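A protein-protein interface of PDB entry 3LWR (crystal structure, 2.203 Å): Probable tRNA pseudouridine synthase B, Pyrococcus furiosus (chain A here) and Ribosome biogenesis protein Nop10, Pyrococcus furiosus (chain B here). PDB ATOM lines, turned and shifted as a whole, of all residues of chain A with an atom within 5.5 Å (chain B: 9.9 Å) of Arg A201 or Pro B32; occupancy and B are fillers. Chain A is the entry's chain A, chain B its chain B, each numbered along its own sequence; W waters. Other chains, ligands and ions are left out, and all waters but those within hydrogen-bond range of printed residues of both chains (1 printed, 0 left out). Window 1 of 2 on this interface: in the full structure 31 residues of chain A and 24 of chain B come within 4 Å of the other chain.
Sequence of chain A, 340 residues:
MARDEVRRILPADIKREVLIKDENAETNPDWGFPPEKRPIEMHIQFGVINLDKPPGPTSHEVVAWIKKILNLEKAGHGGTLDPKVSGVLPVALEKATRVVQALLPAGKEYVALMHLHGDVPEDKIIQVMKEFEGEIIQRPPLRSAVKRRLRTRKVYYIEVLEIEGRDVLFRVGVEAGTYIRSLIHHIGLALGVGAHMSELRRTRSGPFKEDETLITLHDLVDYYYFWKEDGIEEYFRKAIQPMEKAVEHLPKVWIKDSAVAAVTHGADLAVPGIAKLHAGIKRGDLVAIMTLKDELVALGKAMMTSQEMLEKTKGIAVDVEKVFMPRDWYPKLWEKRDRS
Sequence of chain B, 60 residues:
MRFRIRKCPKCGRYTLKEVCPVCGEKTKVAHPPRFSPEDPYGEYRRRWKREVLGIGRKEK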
ATOM      1  N   ASP A  52      13.060  24.322 -24.587  1.00  0.00           N
ATOM      2  CA  ASP A  52      12.831  23.027 -23.941  1.00  0.00           C
ATOM      3  C   ASP A  52      12.891  21.894 -24.998  1.00  0.00           C
ATOM      4  O   ASP A  52      11.880  21.515 -25.574  1.00  0.00           O
ATOM      5  CB  ASP A  52      11.474  23.026 -23.230  1.00  0.00           C
ATOM      6  CG  ASP A  52      11.309  21.859 -22.261  1.00  0.00           C
ATOM      7  OD1 ASP A  52      12.115  20.901 -22.298  1.00  0.00           O
ATOM      8  OD2 ASP A  52      10.356  21.897 -21.454  1.00  0.00           O
ATOM      9  N   LYS A  53      14.075  21.349 -25.231  1.00  0.00           N
ATOM     10  CA  LYS A  53      14.229  20.287 -26.209  1.00  0.00           C
ATOM     11  C   LYS A  53      13.358  19.074 -25.847  1.00  0.00           C
ATOM     12  O   LYS A  53      13.277  18.689 -24.691  1.00  0.00           O
ATOM     13  CB  LYS A  53      15.696  19.902 -26.348  1.00  0.00           C
ATOM     14  CG  LYS A  53      15.942  18.695 -27.292  1.00  0.00           C
ATOM     15  CD  LYS A  53      17.355  18.133 -27.135  1.00  0.00           C
ATOM     16  CE  LYS A  53      17.550  16.843 -27.972  1.00  0.00           C
ATOM     17  NZ  LYS A  53      16.604  15.745 -27.558  1.00  0.00           N
ATOM     18  N   PRO A  54      12.651  18.521 -26.839  1.00  0.00           N
ATOM     19  CA  PRO A  54      11.855  17.296 -26.665  1.00  0.00           C
ATOM     20  C   PRO A  54      12.760  16.079 -26.794  1.00  0.00           C
ATOM     21  O   PRO A  54      13.777  16.157 -27.479  1.00  0.00           O
ATOM     22  CB  PRO A  54      10.917  17.301 -27.876  1.00  0.00           C
ATOM     23  CG  PRO A  54      11.553  18.206 -28.885  1.00  0.00           C
ATOM     24  CD  PRO A  54      12.632  19.020 -28.224  1.00  0.00           C
ATOM     25  N   PRO A  55      12.385  14.955 -26.170  1.00  0.00           N
ATOM     26  CA  PRO A  55      13.127  13.723 -26.462  1.00  0.00           C
ATOM     27  C   PRO A  55      12.895  13.288 -27.919  1.00  0.00           C
ATOM     28  O   PRO A  55      11.832  13.556 -28.471  1.00  0.00           O
ATOM     29  CB  PRO A  55      12.514  12.692 -25.513  1.00  0.00           C
ATOM     30  CG  PRO A  55      11.368  13.372 -24.825  1.00  0.00           C
ATOM     31  CD  PRO A  55      11.131  14.701 -25.457  1.00  0.00           C
ATOM     32  N   VAL A  85      17.284  13.000 -24.450  1.00  0.00           N
ATOM     33  CA  VAL A  85      17.279  13.892 -23.289  1.00  0.00           C
ATOM     34  C   VAL A  85      16.419  15.146 -23.539  1.00  0.00           C
ATOM     35  O   VAL A  85      16.445  15.710 -24.634  1.00  0.00           O
ATOM     36  CB  VAL A  85      18.719  14.289 -22.927  1.00  0.00           C
ATOM     37  CG1 VAL A  85      18.745  15.196 -21.695  1.00  0.00           C
ATOM     38  CG2 VAL A  85      19.566  13.030 -22.683  1.00  0.00           C
ATOM     39  N   SER A  86      15.663  15.581 -22.537  1.00  0.00           N
ATOM     40  CA  SER A  86      14.830  16.773 -22.705  1.00  0.00           C
ATOM     41  C   SER A  86      15.423  17.939 -21.929  1.00  0.00           C
ATOM     42  O   SER A  86      16.397  17.765 -21.204  1.00  0.00           O
ATOM     43  CB  SER A  86      13.391  16.521 -22.258  1.00  0.00           C
ATOM     44  OG  SER A  86      13.288  16.499 -20.846  1.00  0.00           O
ATOM     45  N   GLY A  87      14.864  19.135 -22.112  1.00  0.00           N
ATOM     46  CA  GLY A  87      15.213  20.246 -21.246  1.00  0.00           C
ATOM     47  C   GLY A  87      16.041  21.365 -21.826  1.00  0.00           C
ATOM     48  O   GLY A  87      16.069  21.585 -23.036  1.00  0.00           O
ATOM     49  N   GLU A 109      22.626  21.644 -14.604  1.00  0.00           N
ATOM     50  CA  GLU A 109      21.895  20.835 -13.646  1.00  0.00           C
ATOM     51  C   GLU A 109      20.958  19.905 -14.403  1.00  0.00           C
ATOM     52  O   GLU A 109      20.473  20.248 -15.495  1.00  0.00           O
ATOM     53  CB  GLU A 109      21.152  21.724 -12.659  1.00  0.00           C
ATOM     54  CG  GLU A 109      20.306  21.003 -11.649  1.00  0.00           C
ATOM     55  CD  GLU A 109      19.420  21.969 -10.873  1.00  0.00           C
ATOM     56  OE1 GLU A 109      19.953  22.942 -10.286  1.00  0.00           O
ATOM     57  OE2 GLU A 109      18.189  21.764 -10.867  1.00  0.00           O
ATOM     58  N   TYR A 110      20.754  18.708 -13.844  1.00  0.00           N
ATOM     59  CA  TYR A 110      19.896  17.678 -14.444  1.00  0.00           C
ATOM     60  C   TYR A 110      19.028  17.018 -13.385  1.00  0.00           C
ATOM     61  O   TYR A 110      19.425  16.915 -12.226  1.00  0.00           O
ATOM     62  CB  TYR A 110      20.742  16.560 -15.072  1.00  0.00           C
ATOM     63  CG  TYR A 110      21.673  16.987 -16.176  1.00  0.00           C
ATOM     64  CD1 TYR A 110      22.942  17.477 -15.899  1.00  0.00           C
ATOM     65  CD2 TYR A 110      21.284  16.887 -17.503  1.00  0.00           C
ATOM     66  CE1 TYR A 110      23.800  17.867 -16.932  1.00  0.00           C
ATOM     67  CE2 TYR A 110      22.130  17.259 -18.529  1.00  0.00           C
ATOM     68  CZ  TYR A 110      23.376  17.758 -18.244  1.00  0.00           C
ATOM     69  OH  TYR A 110      24.190  18.125 -19.288  1.00  0.00           O
ATOM     70  N   VAL A 111      17.865  16.534 -13.795  1.00  0.00           N
ATOM     71  CA  VAL A 111      17.109  15.588 -12.988  1.00  0.00           C
ATOM     72  C   VAL A 111      17.253  14.283 -13.738  1.00  0.00           C
ATOM     73  O   VAL A 111      17.065  14.251 -14.953  1.00  0.00           O
ATOM     74  CB  VAL A 111      15.621  15.969 -12.888  1.00  0.00           C
ATOM     75  CG1 VAL A 111      14.837  14.873 -12.172  1.00  0.00           C
ATOM     76  CG2 VAL A 111      15.471  17.291 -12.139  1.00  0.00           C
ATOM     77  N   ALA A 112      17.636  13.215 -13.048  1.00  0.00           N
ATOM     78  CA  ALA A 112      17.895  11.958 -13.730  1.00  0.00           C
ATOM     79  C   ALA A 112      17.177  10.813 -13.055  1.00  0.00           C
ATOM     80  O   ALA A 112      16.970  10.837 -11.849  1.00  0.00           O
ATOM     81  CB  ALA A 112      19.391  11.688 -13.780  1.00  0.00           C
ATOM     82  N   GLU A 199      16.387   7.774 -17.820  1.00  0.00           N
ATOM     83  CA  GLU A 199      15.727   9.030 -18.199  1.00  0.00           C
ATOM     84  C   GLU A 199      16.554  10.234 -17.736  1.00  0.00           C
ATOM     85  O   GLU A 199      17.101  10.216 -16.636  1.00  0.00           O
ATOM     86  CB  GLU A 199      14.329   9.060 -17.573  1.00  0.00           C
ATOM     87  CG  GLU A 199      13.329   9.968 -18.223  1.00  0.00           C
ATOM     88  CD  GLU A 199      11.890   9.630 -17.828  1.00  0.00           C
ATOM     89  OE1 GLU A 199      11.595   8.448 -17.521  1.00  0.00           O
ATOM     90  OE2 GLU A 199      11.041  10.543 -17.839  1.00  0.00           O
ATOM     91  N   LEU A 200      16.666  11.260 -18.577  1.00  0.00           N
ATOM     92  CA  LEU A 200      17.468  12.440 -18.260  1.00  0.00           C
ATOM     93  C   LEU A 200      16.814  13.725 -18.744  1.00  0.00           C
ATOM     94  O   LEU A 200      16.269  13.782 -19.841  1.00  0.00           O
ATOM     95  CB  LEU A 200      18.873  12.317 -18.850  1.00  0.00           C
ATOM     96  CG  LEU A 200      19.854  13.435 -18.482  1.00  0.00           C
ATOM     97  CD1 LEU A 200      20.064  13.505 -16.980  1.00  0.00           C
ATOM     98  CD2 LEU A 200      21.184  13.252 -19.197  1.00  0.00           C
ATOM     99  N   ARG A 201      16.874  14.759 -17.919  1.00  0.00           N
ATOM    100  CA  ARG A 201      16.330  16.048 -18.281  1.00  0.00           C
ATOM    101  C   ARG A 201      17.223  17.148 -17.731  1.00  0.00           C
ATOM    102  O   ARG A 201      17.468  17.209 -16.528  1.00  0.00           O
ATOM    103  CB  ARG A 201      14.898  16.216 -17.755  1.00  0.00           C
ATOM    104  CG  ARG A 201      14.374  17.665 -17.857  1.00  0.00           C
ATOM    105  CD  ARG A 201      12.848  17.739 -17.716  1.00  0.00           C
ATOM    106  NE  ARG A 201      12.374  19.117 -17.839  1.00  0.00           N
ATOM    107  CZ  ARG A 201      12.013  19.675 -18.993  1.00  0.00           C
ATOM    108  NH1 ARG A 201      12.068  18.980 -20.124  1.00  0.00           N
ATOM    109  NH2 ARG A 201      11.589  20.931 -19.029  1.00  0.00           N
ATOM    110  N   ARG A 202      17.703  18.021 -18.613  1.00  0.00           N
ATOM    111  CA  ARG A 202      18.491  19.166 -18.180  1.00  0.00           C
ATOM    112  C   ARG A 202      17.579  20.296 -17.707  1.00  0.00           C
ATOM    113  O   ARG A 202      16.708  20.753 -18.449  1.00  0.00           O
ATOM    114  CB  ARG A 202      19.371  19.673 -19.317  1.00  0.00           C
ATOM    115  CG  ARG A 202      20.408  20.684 -18.864  1.00  0.00           C
ATOM    116  CD  ARG A 202      20.884  21.481 -20.040  1.00  0.00           C
ATOM    117  NE  ARG A 202      22.200  21.063 -20.441  1.00  0.00           N
ATOM    118  CZ  ARG A 202      22.709  21.245 -21.649  1.00  0.00           C
ATOM    119  NH1 ARG A 202      22.003  21.824 -22.606  1.00  0.00           N
ATOM    120  NH2 ARG A 202      23.935  20.824 -21.892  1.00  0.00           N
ATOM    121  N   THR A 203      17.786  20.735 -16.473  1.00  0.00           N
ATOM    122  CA  THR A 203      16.953  21.766 -15.865  1.00  0.00           C
ATOM    123  C   THR A 203      17.676  23.104 -15.740  1.00  0.00           C
ATOM    124  O   THR A 203      17.090  24.095 -15.325  1.00  0.00           O
ATOM    125  CB  THR A 203      16.558  21.377 -14.433  1.00  0.00           C
ATOM    126  OG1 THR A 203      17.751  21.115 -13.695  1.00  0.00           O
ATOM    127  CG2 THR A 203      15.672  20.142 -14.420  1.00  0.00           C
ATOM    128  N   GLU A 210      14.748  26.581 -15.657  1.00  0.00           N
ATOM    129  CA  GLU A 210      13.354  26.238 -15.907  1.00  0.00           C
ATOM    130  C   GLU A 210      12.426  27.301 -15.360  1.00  0.00           C
ATOM    131  O   GLU A 210      11.926  27.179 -14.249  1.00  0.00           O
ATOM    132  CB  GLU A 210      12.997  24.908 -15.246  1.00  0.00           C
ATOM    133  CG  GLU A 210      13.350  23.692 -16.016  1.00  0.00           C
ATOM    134  CD  GLU A 210      12.492  22.512 -15.563  1.00  0.00           C
ATOM    135  OE1 GLU A 210      12.782  21.967 -14.475  1.00  0.00           O
ATOM    136  OE2 GLU A 210      11.506  22.175 -16.271  1.00  0.00           O
ATOM    137  N   LEU A 214      11.388  29.358 -20.494  1.00  0.00           N
ATOM    138  CA  LEU A 214      11.685  28.048 -21.071  1.00  0.00           C
ATOM    139  C   LEU A 214      10.511  27.692 -21.964  1.00  0.00           C
ATOM    140  O   LEU A 214       9.397  27.541 -21.486  1.00  0.00           O
ATOM    141  CB  LEU A 214      11.888  26.974 -19.983  1.00  0.00           C
ATOM    142  CG  LEU A 214      12.236  25.566 -20.476  1.00  0.00           C
ATOM    143  CD1 LEU A 214      13.569  25.580 -21.202  1.00  0.00           C
ATOM    144  CD2 LEU A 214      12.251  24.553 -19.327  1.00  0.00           C
ATOM    145  N   THR A 216       8.724  25.437 -25.257  1.00  0.00           N
ATOM    146  CA  THR A 216       8.675  24.293 -26.158  1.00  0.00           C
ATOM    147  C   THR A 216       8.640  24.694 -27.635  1.00  0.00           C
ATOM    148  O   THR A 216       8.356  25.863 -27.976  1.00  0.00           O
ATOM    149  CB  THR A 216       7.425  23.435 -25.868  1.00  0.00           C
ATOM    150  OG1 THR A 216       6.254  24.185 -26.206  1.00  0.00           O
ATOM    151  CG2 THR A 216       7.347  23.043 -24.372  1.00  0.00           C
ATOM    152  N   PHE B   3       7.571   7.407 -20.235  1.00  0.00           N
ATOM    153  CA  PHE B   3       8.317   8.393 -19.456  1.00  0.00           C
ATOM    154  C   PHE B   3       7.780   8.470 -18.040  1.00  0.00           C
ATOM    155  O   PHE B   3       6.567   8.522 -17.821  1.00  0.00           O
ATOM    156  CB  PHE B   3       8.258   9.775 -20.108  1.00  0.00           C
ATOM    157  CG  PHE B   3       8.969   9.850 -21.426  1.00  0.00           C
ATOM    158  CD1 PHE B   3       8.319  10.335 -22.555  1.00  0.00           C
ATOM    159  CD2 PHE B   3      10.287   9.427 -21.541  1.00  0.00           C
ATOM    160  CE1 PHE B   3       8.972  10.403 -23.777  1.00  0.00           C
ATOM    161  CE2 PHE B   3      10.950   9.489 -22.755  1.00  0.00           C
ATOM    162  CZ  PHE B   3      10.291   9.973 -23.875  1.00  0.00           C
ATOM    163  N   ARG B   4       8.682   8.489 -17.072  1.00  0.00           N
ATOM    164  CA  ARG B   4       8.254   8.382 -15.696  1.00  0.00           C
ATOM    165  C   ARG B   4       8.453   9.657 -14.873  1.00  0.00           C
ATOM    166  O   ARG B   4       7.713   9.898 -13.930  1.00  0.00           O
ATOM    167  CB  ARG B   4       8.936   7.188 -15.044  1.00  0.00           C
ATOM    168  CG  ARG B   4       8.697   5.882 -15.804  1.00  0.00           C
ATOM    169  CD  ARG B   4       9.053   4.697 -14.949  1.00  0.00           C
ATOM    170  NE  ARG B   4       8.619   4.893 -13.568  1.00  0.00           N
ATOM    171  CZ  ARG B   4       9.186   4.296 -12.527  1.00  0.00           C
ATOM    172  NH1 ARG B   4      10.208   3.475 -12.727  1.00  0.00           N
ATOM    173  NH2 ARG B   4       8.747   4.524 -11.295  1.00  0.00           N
ATOM    174  N   ILE B   5       9.441  10.471 -15.228  1.00  0.00           N
ATOM    175  CA  ILE B   5       9.697  11.700 -14.490  1.00  0.00           C
ATOM    176  C   ILE B   5       8.525  12.662 -14.626  1.00  0.00           C
ATOM    177  O   ILE B   5       8.092  12.990 -15.742  1.00  0.00           O
ATOM    178  CB  ILE B   5      10.982  12.363 -14.977  1.00  0.00           C
ATOM    179  CG1 ILE B   5      12.163  11.413 -14.749  1.00  0.00           C
ATOM    180  CG2 ILE B   5      11.195  13.691 -14.266  1.00  0.00           C
ATOM    181  CD1 ILE B   5      13.505  11.945 -15.287  1.00  0.00           C
ATOM    182  N   ARG B   6       7.988  13.090 -13.495  1.00  0.00           N
ATOM    183  CA  ARG B   6       6.890  14.047 -13.496  1.00  0.00           C
ATOM    184  C   ARG B   6       7.308  15.305 -12.741  1.00  0.00           C
ATOM    185  O   ARG B   6       8.284  15.292 -11.999  1.00  0.00           O
ATOM    186  CB  ARG B   6       5.661  13.427 -12.839  1.00  0.00           C
ATOM    187  CG  ARG B   6       5.311  12.048 -13.411  1.00  0.00           C
ATOM    188  CD  ARG B   6       4.057  11.486 -12.770  1.00  0.00           C
ATOM    189  NE  ARG B   6       2.894  12.310 -13.073  1.00  0.00           N
ATOM    190  CZ  ARG B   6       2.132  12.142 -14.145  1.00  0.00           C
ATOM    191  NH1 ARG B   6       2.409  11.175 -15.010  1.00  0.00           N
ATOM    192  NH2 ARG B   6       1.092  12.935 -14.347  1.00  0.00           N
ATOM    193  N   LYS B   7       6.580  16.393 -12.939  1.00  0.00           N
ATOM    194  CA  LYS B   7       6.796  17.591 -12.141  1.00  0.00           C
ATOM    195  C   LYS B   7       5.513  18.321 -11.748  1.00  0.00           C
ATOM    196  O   LYS B   7       4.535  18.345 -12.491  1.00  0.00           O
ATOM    197  CB  LYS B   7       7.821  18.538 -12.768  1.00  0.00           C
ATOM    198  CG  LYS B   7       7.559  18.953 -14.176  1.00  0.00           C
ATOM    199  CD  LYS B   7       8.033  20.409 -14.367  1.00  0.00           C
ATOM    200  CE  LYS B   7       9.105  20.783 -13.363  1.00  0.00           C
ATOM    201  NZ  LYS B   7       9.333  22.258 -13.314  1.00  0.00           N
ATOM    202  N   GLY B  12       6.960  22.985  -8.676  1.00  0.00           N
ATOM    203  CA  GLY B  12       8.200  22.820  -9.427  1.00  0.00           C
ATOM    204  C   GLY B  12       8.907  21.511  -9.000  1.00  0.00           C
ATOM    205  O   GLY B  12       9.927  21.107  -9.545  1.00  0.00           O
ATOM    206  N   ARG B  13       8.353  20.839  -8.004  1.00  0.00           N
ATOM    207  CA  ARG B  13       8.940  19.591  -7.506  1.00  0.00           C
ATOM    208  C   ARG B  13       8.961  18.475  -8.575  1.00  0.00           C
ATOM    209  O   ARG B  13       7.971  18.257  -9.289  1.00  0.00           O
ATOM    210  CB  ARG B  13       8.175  19.139  -6.268  1.00  0.00           C
ATOM    211  CG  ARG B  13       8.443  17.713  -5.840  1.00  0.00           C
ATOM    212  CD  ARG B  13       9.707  17.580  -5.010  1.00  0.00           C
ATOM    213  NE  ARG B  13       9.885  16.176  -4.631  1.00  0.00           N
ATOM    214  CZ  ARG B  13      10.510  15.750  -3.540  1.00  0.00           C
ATOM    215  NH1 ARG B  13      11.039  16.616  -2.683  1.00  0.00           N
ATOM    216  NH2 ARG B  13      10.605  14.445  -3.310  1.00  0.00           N
ATOM    217  N   TYR B  14      10.100  17.790  -8.698  1.00  0.00           N
ATOM    218  CA  TYR B  14      10.204  16.608  -9.549  1.00  0.00           C
ATOM    219  C   TYR B  14       9.891  15.369  -8.720  1.00  0.00           C
ATOM    220  O   TYR B  14      10.395  15.209  -7.613  1.00  0.00           O
ATOM    221  CB  TYR B  14      11.600  16.505 -10.171  1.00  0.00           C
ATOM    222  CG  TYR B  14      11.747  17.349 -11.415  1.00  0.00           C
ATOM    223  CD1 TYR B  14      12.343  18.600 -11.372  1.00  0.00           C
ATOM    224  CD2 TYR B  14      11.249  16.900 -12.626  1.00  0.00           C
ATOM    225  CE1 TYR B  14      12.456  19.372 -12.516  1.00  0.00           C
ATOM    226  CE2 TYR B  14      11.352  17.648 -13.753  1.00  0.00           C
ATOM    227  CZ  TYR B  14      11.950  18.881 -13.704  1.00  0.00           C
ATOM    228  OH  TYR B  14      12.029  19.596 -14.871  1.00  0.00           O
ATOM    229  N   THR B  15       9.085  14.474  -9.266  1.00  0.00           N
ATOM    230  CA  THR B  15       8.576  13.359  -8.488  1.00  0.00           C
ATOM    231  C   THR B  15       8.202  12.294  -9.496  1.00  0.00           C
ATOM    232  O   THR B  15       8.050  12.612 -10.678  1.00  0.00           O
ATOM    233  CB  THR B  15       7.319  13.811  -7.669  1.00  0.00           C
ATOM    234  OG1 THR B  15       6.727  12.695  -7.009  1.00  0.00           O
ATOM    235  CG2 THR B  15       6.256  14.432  -8.580  1.00  0.00           C
ATOM    236  N   LYS B  28       2.366  16.576 -13.648  1.00  0.00           N
ATOM    237  CA  LYS B  28       2.352  16.355 -15.089  1.00  0.00           C
ATOM    238  C   LYS B  28       3.687  15.795 -15.579  1.00  0.00           C
ATOM    239  O   LYS B  28       4.732  16.067 -14.986  1.00  0.00           O
ATOM    240  CB  LYS B  28       2.051  17.675 -15.814  1.00  0.00           C
ATOM    241  CG  LYS B  28       0.657  18.210 -15.510  1.00  0.00           C
ATOM    242  CD  LYS B  28       0.291  19.382 -16.408  1.00  0.00           C
ATOM    243  CE  LYS B  28      -1.191  19.721 -16.287  1.00  0.00           C
ATOM    244  NZ  LYS B  28      -1.592  20.825 -17.203  1.00  0.00           N
ATOM    245  N   VAL B  29       3.634  15.027 -16.671  1.00  0.00           N
ATOM    246  CA  VAL B  29       4.823  14.519 -17.345  1.00  0.00           C
ATOM    247  C   VAL B  29       5.833  15.641 -17.595  1.00  0.00           C
ATOM    248  O   VAL B  29       5.475  16.703 -18.113  1.00  0.00           O
ATOM    249  CB  VAL B  29       4.451  13.884 -18.713  1.00  0.00           C
ATOM    250  CG1 VAL B  29       5.702  13.366 -19.423  1.00  0.00           C
ATOM    251  CG2 VAL B  29       3.426  12.777 -18.528  1.00  0.00           C
ATOM    252  N   ALA B  30       7.095  15.384 -17.271  1.00  0.00           N
ATOM    253  CA  ALA B  30       8.125  16.424 -17.268  1.00  0.00           C
ATOM    254  C   ALA B  30       8.696  16.767 -18.639  1.00  0.00           C
ATOM    255  O   ALA B  30       9.122  17.892 -18.872  1.00  0.00           O
ATOM    256  CB  ALA B  30       9.243  16.051 -16.310  1.00  0.00           C
ATOM    257  N   HIS B  31       8.708  15.808 -19.550  1.00  0.00           N
ATOM    258  CA  HIS B  31       9.193  16.065 -20.909  1.00  0.00           C
ATOM    259  C   HIS B  31       8.136  16.786 -21.756  1.00  0.00           C
ATOM    260  O   HIS B  31       6.944  16.542 -21.586  1.00  0.00           O
ATOM    261  CB  HIS B  31       9.611  14.733 -21.553  1.00  0.00           C
ATOM    262  CG  HIS B  31      10.556  13.948 -20.701  1.00  0.00           C
ATOM    263  ND1 HIS B  31      11.927  14.089 -20.783  1.00  0.00           N
ATOM    264  CD2 HIS B  31      10.328  13.066 -19.699  1.00  0.00           C
ATOM    265  CE1 HIS B  31      12.503  13.304 -19.892  1.00  0.00           C
ATOM    266  NE2 HIS B  31      11.556  12.676 -19.218  1.00  0.00           N
ATOM    267  N   PRO B  32       8.569  17.692 -22.655  1.00  0.00           N
ATOM    268  CA  PRO B  32       7.664  18.354 -23.605  1.00  0.00           C
ATOM    269  C   PRO B  32       7.155  17.353 -24.635  1.00  0.00           C
ATOM    270  O   PRO B  32       7.821  16.349 -24.851  1.00  0.00           O
ATOM    271  CB  PRO B  32       8.571  19.370 -24.344  1.00  0.00           C
ATOM    272  CG  PRO B  32       9.890  19.291 -23.721  1.00  0.00           C
ATOM    273  CD  PRO B  32       9.973  18.083 -22.855  1.00  0.00           C
ATOM    274  N   PRO B  33       6.027  17.656 -25.303  1.00  0.00           N
ATOM    275  CA  PRO B  33       5.470  16.758 -26.321  1.00  0.00           C
ATOM    276  C   PRO B  33       6.414  16.667 -27.506  1.00  0.00           C
ATOM    277  O   PRO B  33       7.097  17.639 -27.833  1.00  0.00           O
ATOM    278  CB  PRO B  33       4.180  17.468 -26.759  1.00  0.00           C
ATOM    279  CG  PRO B  33       3.920  18.523 -25.705  1.00  0.00           C
ATOM    280  CD  PRO B  33       5.256  18.903 -25.185  1.00  0.00           C
ATOM    281  N   ARG B  34       6.451  15.518 -28.163  1.00  0.00           N
ATOM    282  CA  ARG B  34       7.316  15.382 -29.324  1.00  0.00           C
ATOM    283  C   ARG B  34       6.837  16.300 -30.458  1.00  0.00           C
ATOM    284  O   ARG B  34       5.647  16.555 -30.595  1.00  0.00           O
ATOM    285  CB  ARG B  34       7.406  13.910 -29.729  1.00  0.00           C
ATOM    286  CG  ARG B  34       7.869  13.037 -28.540  1.00  0.00           C
ATOM    287  CD  ARG B  34       7.829  11.538 -28.824  1.00  0.00           C
ATOM    288  NE  ARG B  34       9.121  11.051 -29.295  1.00  0.00           N
ATOM    289  CZ  ARG B  34      10.056  10.518 -28.510  1.00  0.00           C
ATOM    290  NH1 ARG B  34       9.848  10.395 -27.203  1.00  0.00           N
ATOM    291  NH2 ARG B  34      11.200  10.108 -29.036  1.00  0.00           N
ATOM    292  N   PHE B  35       7.770  16.821 -31.244  1.00  0.00           N
ATOM    293  CA  PHE B  35       7.441  17.808 -32.272  1.00  0.00           C
ATOM    294  C   PHE B  35       7.931  17.323 -33.626  1.00  0.00           C
ATOM    295  O   PHE B  35       9.009  16.726 -33.703  1.00  0.00           O
ATOM    296  CB  PHE B  35       8.097  19.157 -31.934  1.00  0.00           C
ATOM    297  CG  PHE B  35       7.850  20.239 -32.957  1.00  0.00           C
ATOM    298  CD1 PHE B  35       6.715  21.030 -32.889  1.00  0.00           C
ATOM    299  CD2 PHE B  35       8.753  20.462 -33.983  1.00  0.00           C
ATOM    300  CE1 PHE B  35       6.477  22.015 -33.827  1.00  0.00           C
ATOM    301  CE2 PHE B  35       8.529  21.462 -34.931  1.00  0.00           C
ATOM    302  CZ  PHE B  35       7.386  22.233 -34.848  1.00  0.00           C
HETATM  303  O   HOH W   1       8.577  20.121 -20.462  1.00  0.00           O
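OD1 of Asp A52 touches CG of Pro B32 (3.1 Å).
Lys A53 touches Pro B32 (O to CG, 3.6 Å).
O of Pro B33 touches CB of Pro A54, 3.8 Å away.
Pro A55 touches Phe B3.
Pro A55 touches His B31.
Tyr B14 touches Val A111.
OE2 of Glu A199 touches CB of Phe B3 (3.7 Å).
OH of Tyr B14 touches CG2 of Thr A203, at 3.7 Å.
Of chain B, only Tyr B14, Ala B30 and Pro B32 come within 4 Å of Arg A201.
Of the printed residues of chain B, Ser A86 touches His B31 (2.8 Å) and Pro B32 (3.8 Å).
No residue of chain B comes within 4 Å of Gly A87.
Of chain B, only Tyr B14 (3.5 Å) comes within 4 Å of Val A111.
Leu A200 touches just one residue of chain B: His B31.
Of the printed residues of chain B, Glu A210 touches Lys B7 and Tyr B14.
Of the printed residues of chain A, Arg B4 touches Glu A199.
Printed residues of chain B within 4 Å of Thr A216: Pro B32.
Tyr A110 touches none of the printed residues of chain B.
The nearest residue of chain A that does not touch Pro B32 is Pro A54 (4.1 Å).
The backbone carbonyl oxygen (O) of Leu A200 lies within hydrogen-bond range of the backbone NH (N) of Ser A86.
NH1 of Arg A201 sits at hydrogen-bond distance from OG of Ser A86 (2.9 Å).
The backbone carbonyl oxygen (O) of Thr A203 is in hydrogen-bond range of the backbone NH (N) of Glu A210, 3.4 Å away.
Of the 17 printed residues of chain B, 10 touch a printed residue of chain A.
Of the 19 printed residues of chain A, 12 touch a printed residue of chain B.
Hydrophobic or aromatic side chains of chain A within 4 Å of the printed part of chain B: Pro A54, Pro A55 and Val A111.
Among the printed residues, 22 pairs touch across the chains.
Water W1 lies within hydrogen-bond range of OD2 of Asp A52, O of Ala B30 and NH2 of Arg A201.
A ring nitrogen (ND1) of His B31 lies within hydrogen-bond range of the side-chain hydroxyl of Ser A86, at 2.8 Å.
The side-chain carboxylate (OE1) of Glu A199 lies within hydrogen-bond range of the backbone NH (N) of Arg B4 (2.9 Å).
N of Ile B5 sits at hydrogen-bond distance from OE2 of Glu A199, at 3.1 Å.
The side-chain carboxylate (OE2) of Glu A199 sits at hydrogen-bond distance from a ring nitrogen (NE2) of His B31 (2.6 Å).
The guanidinium group (NE) of Arg A201 is in hydrogen-bond range of the side-chain hydroxyl (OH) of Tyr B14 (3.0 Å).
The guanidinium group (NH1) of Arg A201 lies within hydrogen-bond range of the backbone carbonyl oxygen (O) of Ala B30 (3.4 Å).
NZ of Lys B7 is in salt-bridge range of OE1 of Glu A210 (3.7 Å).
The side-chain carboxylate (OE1) of Glu A210 is in hydrogen-bond range of the side-chain hydroxyl (OH) of Tyr B14 (2.5 Å).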
